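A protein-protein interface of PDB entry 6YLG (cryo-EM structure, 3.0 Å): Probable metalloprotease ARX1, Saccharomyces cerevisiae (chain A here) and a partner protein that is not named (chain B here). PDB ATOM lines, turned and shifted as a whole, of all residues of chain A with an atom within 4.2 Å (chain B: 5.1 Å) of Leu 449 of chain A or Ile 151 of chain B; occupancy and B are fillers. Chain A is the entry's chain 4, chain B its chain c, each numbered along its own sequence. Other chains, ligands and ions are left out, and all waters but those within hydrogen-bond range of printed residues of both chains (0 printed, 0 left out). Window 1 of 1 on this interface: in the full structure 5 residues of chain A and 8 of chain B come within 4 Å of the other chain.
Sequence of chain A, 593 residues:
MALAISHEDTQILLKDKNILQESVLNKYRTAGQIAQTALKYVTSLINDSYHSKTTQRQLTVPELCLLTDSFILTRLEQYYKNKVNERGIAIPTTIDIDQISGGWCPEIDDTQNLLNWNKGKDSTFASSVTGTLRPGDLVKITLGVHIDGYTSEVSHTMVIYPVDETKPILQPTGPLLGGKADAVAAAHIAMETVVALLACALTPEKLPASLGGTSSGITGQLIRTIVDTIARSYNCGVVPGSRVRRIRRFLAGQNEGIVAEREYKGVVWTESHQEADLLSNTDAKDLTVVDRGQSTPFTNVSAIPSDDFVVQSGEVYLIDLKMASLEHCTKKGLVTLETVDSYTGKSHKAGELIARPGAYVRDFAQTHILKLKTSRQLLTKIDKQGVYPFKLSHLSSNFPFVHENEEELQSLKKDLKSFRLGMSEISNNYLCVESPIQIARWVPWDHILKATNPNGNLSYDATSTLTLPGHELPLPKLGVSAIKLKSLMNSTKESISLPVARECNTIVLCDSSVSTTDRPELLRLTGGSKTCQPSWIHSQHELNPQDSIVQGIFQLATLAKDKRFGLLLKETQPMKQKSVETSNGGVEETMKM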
ATOM      1  N   LYS A 332      10.887  10.518 -12.857  1.00  0.00           N
ATOM      2  CA  LYS A 332       9.458  10.396 -12.628  1.00  0.00           C
ATOM      3  C   LYS A 332       8.731  11.548 -13.310  1.00  0.00           C
ATOM      4  O   LYS A 332       9.206  12.685 -13.347  1.00  0.00           O
ATOM      5  CB  LYS A 332       9.143  10.395 -11.131  1.00  0.00           C
ATOM      6  CG  LYS A 332       8.963   9.013 -10.516  1.00  0.00           C
ATOM      7  CD  LYS A 332      10.297   8.406 -10.107  1.00  0.00           C
ATOM      8  CE  LYS A 332      10.814   8.974  -8.790  1.00  0.00           C
ATOM      9  NZ  LYS A 332      11.814   8.072  -8.163  1.00  0.00           N
ATOM     10  N   TRP A 445       7.683  15.934 -12.955  1.00  0.00           N
ATOM     11  CA  TRP A 445       7.080  16.509 -11.756  1.00  0.00           C
ATOM     12  C   TRP A 445       7.779  17.789 -11.306  1.00  0.00           C
ATOM     13  O   TRP A 445       7.204  18.558 -10.527  1.00  0.00           O
ATOM     14  CB  TRP A 445       7.100  15.484 -10.624  1.00  0.00           C
ATOM     15  CG  TRP A 445       6.106  14.383 -10.793  1.00  0.00           C
ATOM     16  CD1 TRP A 445       6.359  13.107 -11.204  1.00  0.00           C
ATOM     17  CD2 TRP A 445       4.696  14.453 -10.550  1.00  0.00           C
ATOM     18  NE1 TRP A 445       5.195  12.381 -11.238  1.00  0.00           N
ATOM     19  CE2 TRP A 445       4.160  13.185 -10.840  1.00  0.00           C
ATOM     20  CE3 TRP A 445       3.836  15.466 -10.118  1.00  0.00           C
ATOM     21  CZ2 TRP A 445       2.805  12.902 -10.710  1.00  0.00           C
ATOM     22  CZ3 TRP A 445       2.492  15.184  -9.991  1.00  0.00           C
ATOM     23  CH2 TRP A 445       1.989  13.912 -10.286  1.00  0.00           C
ATOM     24  N   ASP A 446       9.011  18.028 -11.765  1.00  0.00           N
ATOM     25  CA  ASP A 446       9.755  19.205 -11.323  1.00  0.00           C
ATOM     26  C   ASP A 446       9.045  20.492 -11.720  1.00  0.00           C
ATOM     27  O   ASP A 446       8.847  21.384 -10.885  1.00  0.00           O
ATOM     28  CB  ASP A 446      11.165  19.176 -11.907  1.00  0.00           C
ATOM     29  CG  ASP A 446      11.960  17.966 -11.453  1.00  0.00           C
ATOM     30  OD1 ASP A 446      11.356  17.050 -10.856  1.00  0.00           O
ATOM     31  OD2 ASP A 446      13.184  17.927 -11.698  1.00  0.00           O
ATOM     32  N   HIS A 447       8.665  20.608 -12.995  1.00  0.00           N
ATOM     33  CA  HIS A 447       7.959  21.798 -13.460  1.00  0.00           C
ATOM     34  C   HIS A 447       6.642  21.981 -12.719  1.00  0.00           C
ATOM     35  O   HIS A 447       6.282  23.100 -12.339  1.00  0.00           O
ATOM     36  CB  HIS A 447       7.713  21.699 -14.965  1.00  0.00           C
ATOM     37  CG  HIS A 447       8.868  22.154 -15.797  1.00  0.00           C
ATOM     38  ND1 HIS A 447      10.011  21.400 -15.956  1.00  0.00           N
ATOM     39  CD2 HIS A 447       9.057  23.282 -16.521  1.00  0.00           C
ATOM     40  CE1 HIS A 447      10.856  22.045 -16.739  1.00  0.00           C
ATOM     41  NE2 HIS A 447      10.301  23.190 -17.097  1.00  0.00           N
ATOM     42  N   ILE A 448       5.922  20.883 -12.484  1.00  0.00           N
ATOM     43  CA  ILE A 448       4.614  20.971 -11.845  1.00  0.00           C
ATOM     44  C   ILE A 448       4.755  21.453 -10.410  1.00  0.00           C
ATOM     45  O   ILE A 448       3.974  22.291  -9.942  1.00  0.00           O
ATOM     46  CB  ILE A 448       3.899  19.608 -11.922  1.00  0.00           C
ATOM     47  CG1 ILE A 448       3.526  19.282 -13.371  1.00  0.00           C
ATOM     48  CG2 ILE A 448       2.660  19.587 -11.030  1.00  0.00           C
ATOM     49  CD1 ILE A 448       3.841  17.864 -13.769  1.00  0.00           C
ATOM     50  N   LEU A 449       5.749  20.937  -9.688  1.00  0.00           N
ATOM     51  CA  LEU A 449       5.905  21.305  -8.286  1.00  0.00           C
ATOM     52  C   LEU A 449       6.490  22.705  -8.146  1.00  0.00           C
ATOM     53  O   LEU A 449       6.200  23.407  -7.170  1.00  0.00           O
ATOM     54  CB  LEU A 449       6.779  20.277  -7.574  1.00  0.00           C
ATOM     55  CG  LEU A 449       6.225  18.851  -7.580  1.00  0.00           C
ATOM     56  CD1 LEU A 449       7.336  17.847  -7.344  1.00  0.00           C
ATOM     57  CD2 LEU A 449       5.124  18.699  -6.555  1.00  0.00           C
ATOM     58  N   LYS A 450       7.314  23.127  -9.107  1.00  0.00           N
ATOM     59  CA  LYS A 450       7.838  24.487  -9.090  1.00  0.00           C
ATOM     60  C   LYS A 450       6.854  25.475  -9.715  1.00  0.00           C
ATOM     61  O   LYS A 450       7.129  26.679  -9.780  1.00  0.00           O
ATOM     62  CB  LYS A 450       9.174  24.530  -9.828  1.00  0.00           C
ATOM     63  CG  LYS A 450      10.314  23.866  -9.083  1.00  0.00           C
ATOM     64  CD  LYS A 450      11.478  23.592 -10.019  1.00  0.00           C
ATOM     65  CE  LYS A 450      12.798  23.517  -9.275  1.00  0.00           C
ATOM     66  NZ  LYS A 450      13.939  23.340 -10.215  1.00  0.00           N
ATOM     67  N   ALA A 451       5.706  24.989 -10.186  1.00  0.00           N
ATOM     68  CA  ALA A 451       4.768  25.841 -10.895  1.00  0.00           C
ATOM     69  C   ALA A 451       4.136  26.865  -9.958  1.00  0.00           C
ATOM     70  O   ALA A 451       4.325  26.847  -8.738  1.00  0.00           O
ATOM     71  CB  ALA A 451       3.673  25.001 -11.545  1.00  0.00           C
ATOM     72  N   LYS B 144       3.208  18.535  -0.935  1.00  0.00           N
ATOM     73  CA  LYS B 144       4.368  18.803  -1.779  1.00  0.00           C
ATOM     74  C   LYS B 144       5.649  18.315  -1.118  1.00  0.00           C
ATOM     75  O   LYS B 144       6.566  17.854  -1.804  1.00  0.00           O
ATOM     76  CB  LYS B 144       4.463  20.293  -2.101  1.00  0.00           C
ATOM     77  CG  LYS B 144       3.698  20.683  -3.351  1.00  0.00           C
ATOM     78  CD  LYS B 144       3.761  22.174  -3.615  1.00  0.00           C
ATOM     79  CE  LYS B 144       3.556  22.479  -5.088  1.00  0.00           C
ATOM     80  NZ  LYS B 144       3.008  23.841  -5.297  1.00  0.00           N
ATOM     81  N   LEU B 147       5.680  14.637  -1.713  1.00  0.00           N
ATOM     82  CA  LEU B 147       5.899  14.355  -3.123  1.00  0.00           C
ATOM     83  C   LEU B 147       7.350  14.586  -3.523  1.00  0.00           C
ATOM     84  O   LEU B 147       7.909  13.785  -4.279  1.00  0.00           O
ATOM     85  CB  LEU B 147       4.953  15.222  -3.963  1.00  0.00           C
ATOM     86  CG  LEU B 147       4.658  14.911  -5.432  1.00  0.00           C
ATOM     87  CD1 LEU B 147       4.570  13.426  -5.734  1.00  0.00           C
ATOM     88  CD2 LEU B 147       3.348  15.584  -5.783  1.00  0.00           C
ATOM     89  N   TRP B 148       7.967  15.668  -3.032  1.00  0.00           N
ATOM     90  CA  TRP B 148       9.406  15.846  -3.169  1.00  0.00           C
ATOM     91  C   TRP B 148      10.164  14.655  -2.606  1.00  0.00           C
ATOM     92  O   TRP B 148      11.117  14.172  -3.234  1.00  0.00           O
ATOM     93  CB  TRP B 148       9.852  17.118  -2.452  1.00  0.00           C
ATOM     94  CG  TRP B 148       9.648  18.385  -3.236  1.00  0.00           C
ATOM     95  CD1 TRP B 148       8.876  19.453  -2.877  1.00  0.00           C
ATOM     96  CD2 TRP B 148      10.232  18.723  -4.500  1.00  0.00           C
ATOM     97  NE1 TRP B 148       8.937  20.427  -3.840  1.00  0.00           N
ATOM     98  CE2 TRP B 148       9.763  20.005  -4.848  1.00  0.00           C
ATOM     99  CE3 TRP B 148      11.103  18.065  -5.372  1.00  0.00           C
ATOM    100  CZ2 TRP B 148      10.134  20.641  -6.028  1.00  0.00           C
ATOM    101  CZ3 TRP B 148      11.469  18.699  -6.547  1.00  0.00           C
ATOM    102  CH2 TRP B 148      10.985  19.974  -6.862  1.00  0.00           C
ATOM    103  N   SER B 149       9.756  14.183  -1.423  1.00  0.00           N
ATOM    104  CA  SER B 149      10.385  13.011  -0.818  1.00  0.00           C
ATOM    105  C   SER B 149      10.327  11.811  -1.749  1.00  0.00           C
ATOM    106  O   SER B 149      11.318  11.090  -1.908  1.00  0.00           O
ATOM    107  CB  SER B 149       9.703  12.683   0.510  1.00  0.00           C
ATOM    108  OG  SER B 149       8.563  11.859   0.313  1.00  0.00           O
ATOM    109  N   VAL B 150       9.176  11.587  -2.377  1.00  0.00           N
ATOM    110  CA  VAL B 150       9.071  10.382  -3.196  1.00  0.00           C
ATOM    111  C   VAL B 150       9.828  10.557  -4.511  1.00  0.00           C
ATOM    112  O   VAL B 150      10.510   9.635  -4.973  1.00  0.00           O
ATOM    113  CB  VAL B 150       7.592  10.015  -3.431  1.00  0.00           C
ATOM    114  CG1 VAL B 150       7.452   8.984  -4.555  1.00  0.00           C
ATOM    115  CG2 VAL B 150       6.975   9.487  -2.140  1.00  0.00           C
ATOM    116  N   ILE B 151       9.815  11.749  -5.115  1.00  0.00           N
ATOM    117  CA  ILE B 151      10.464  11.890  -6.419  1.00  0.00           C
ATOM    118  C   ILE B 151      11.981  11.987  -6.307  1.00  0.00           C
ATOM    119  O   ILE B 151      12.686  11.587  -7.241  1.00  0.00           O
ATOM    120  CB  ILE B 151       9.927  13.093  -7.224  1.00  0.00           C
ATOM    121  CG1 ILE B 151      10.174  14.448  -6.546  1.00  0.00           C
ATOM    122  CG2 ILE B 151       8.438  12.926  -7.478  1.00  0.00           C
ATOM    123  CD1 ILE B 151      10.216  15.595  -7.526  1.00  0.00           C
ATOM    124  N   ASP B 152      12.512  12.508  -5.196  1.00  0.00           N
ATOM    125  CA  ASP B 152      13.959  12.605  -5.056  1.00  0.00           C
ATOM    126  C   ASP B 152      14.624  11.243  -4.892  1.00  0.00           C
ATOM    127  O   ASP B 152      15.842  11.143  -5.074  1.00  0.00           O
ATOM    128  CB  ASP B 152      14.309  13.502  -3.868  1.00  0.00           C
ATOM    129  CG  ASP B 152      13.878  14.942  -4.074  1.00  0.00           C
ATOM    130  OD1 ASP B 152      13.943  15.729  -3.106  1.00  0.00           O
ATOM    131  OD2 ASP B 152      13.468  15.288  -5.202  1.00  0.00           O
ATOM    132  N   ASP B 153      13.860  10.204  -4.559  1.00  0.00           N
ATOM    133  CA  ASP B 153      14.393   8.856  -4.386  1.00  0.00           C
ATOM    134  C   ASP B 153      13.514   7.838  -5.103  1.00  0.00           C
ATOM    135  O   ASP B 153      12.704   8.196  -5.956  1.00  0.00           O
ATOM    136  CB  ASP B 153      14.495   8.509  -2.901  1.00  0.00           C
ATOM    137  CG  ASP B 153      15.521   7.433  -2.623  1.00  0.00           C
ATOM    138  OD1 ASP B 153      16.706   7.776  -2.426  1.00  0.00           O
ATOM    139  OD2 ASP B 153      15.144   6.243  -2.604  1.00  0.00           O
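The backbone carbonyl oxygen (O) of Asp 153 of chain B sits close to the side-chain amino group (NZ) of Lys 332 of chain A.
Lys 332 of chain A touches Val 150 of chain B. O of Ile 151 of chain B touches CE of Lys 332 of chain A, 3.6 Å away. OD1 of Asp 446 of chain A touches CD1 of Ile 151 of chain B, 3.8 Å away. Lys 144 of chain B touches Leu 449 of chain A. CD2 of Leu 147 of chain B touches CD2 of Leu 449 of chain A, at 3.7 Å. Trp 148 of chain B touches Leu 449 of chain A (CZ2 to CB, 3.7 Å). Leu 449 of chain A touches Ile 151 of chain B.
Printed residues of chain A within 4 Å of Trp 148 of chain B: Leu 449 (3.7 Å). Of the printed residues of chain A, Val 150 of chain B touches Lys 332. Printed residues of chain A within 4 Å of Asp 153 of chain B: Lys 332 (2.4 Å). Ile 448 of chain A touches none of the printed residues of chain B. The nearest printed residue of chain A that does not touch Ile 151 of chain B is Trp 445 of chain A (4.3 Å).
Printed residues of chain B that touch a printed residue of chain A: Lys 144, Leu 147, Trp 148, Val 150, Ile 151 and Asp 153. Of the 8 printed residues of chain A, 3 touch a printed residue of chain B. Hydrophobic or aromatic side chains of chain A within 4 Å of the printed part of chain B: Leu 449. Among the printed residues, 8 pairs touch across the chains. Among the printed residues, no Asp or Glu carboxylate lies within 4 Å of a Lys or Arg side-chain nitrogen of the other chain.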
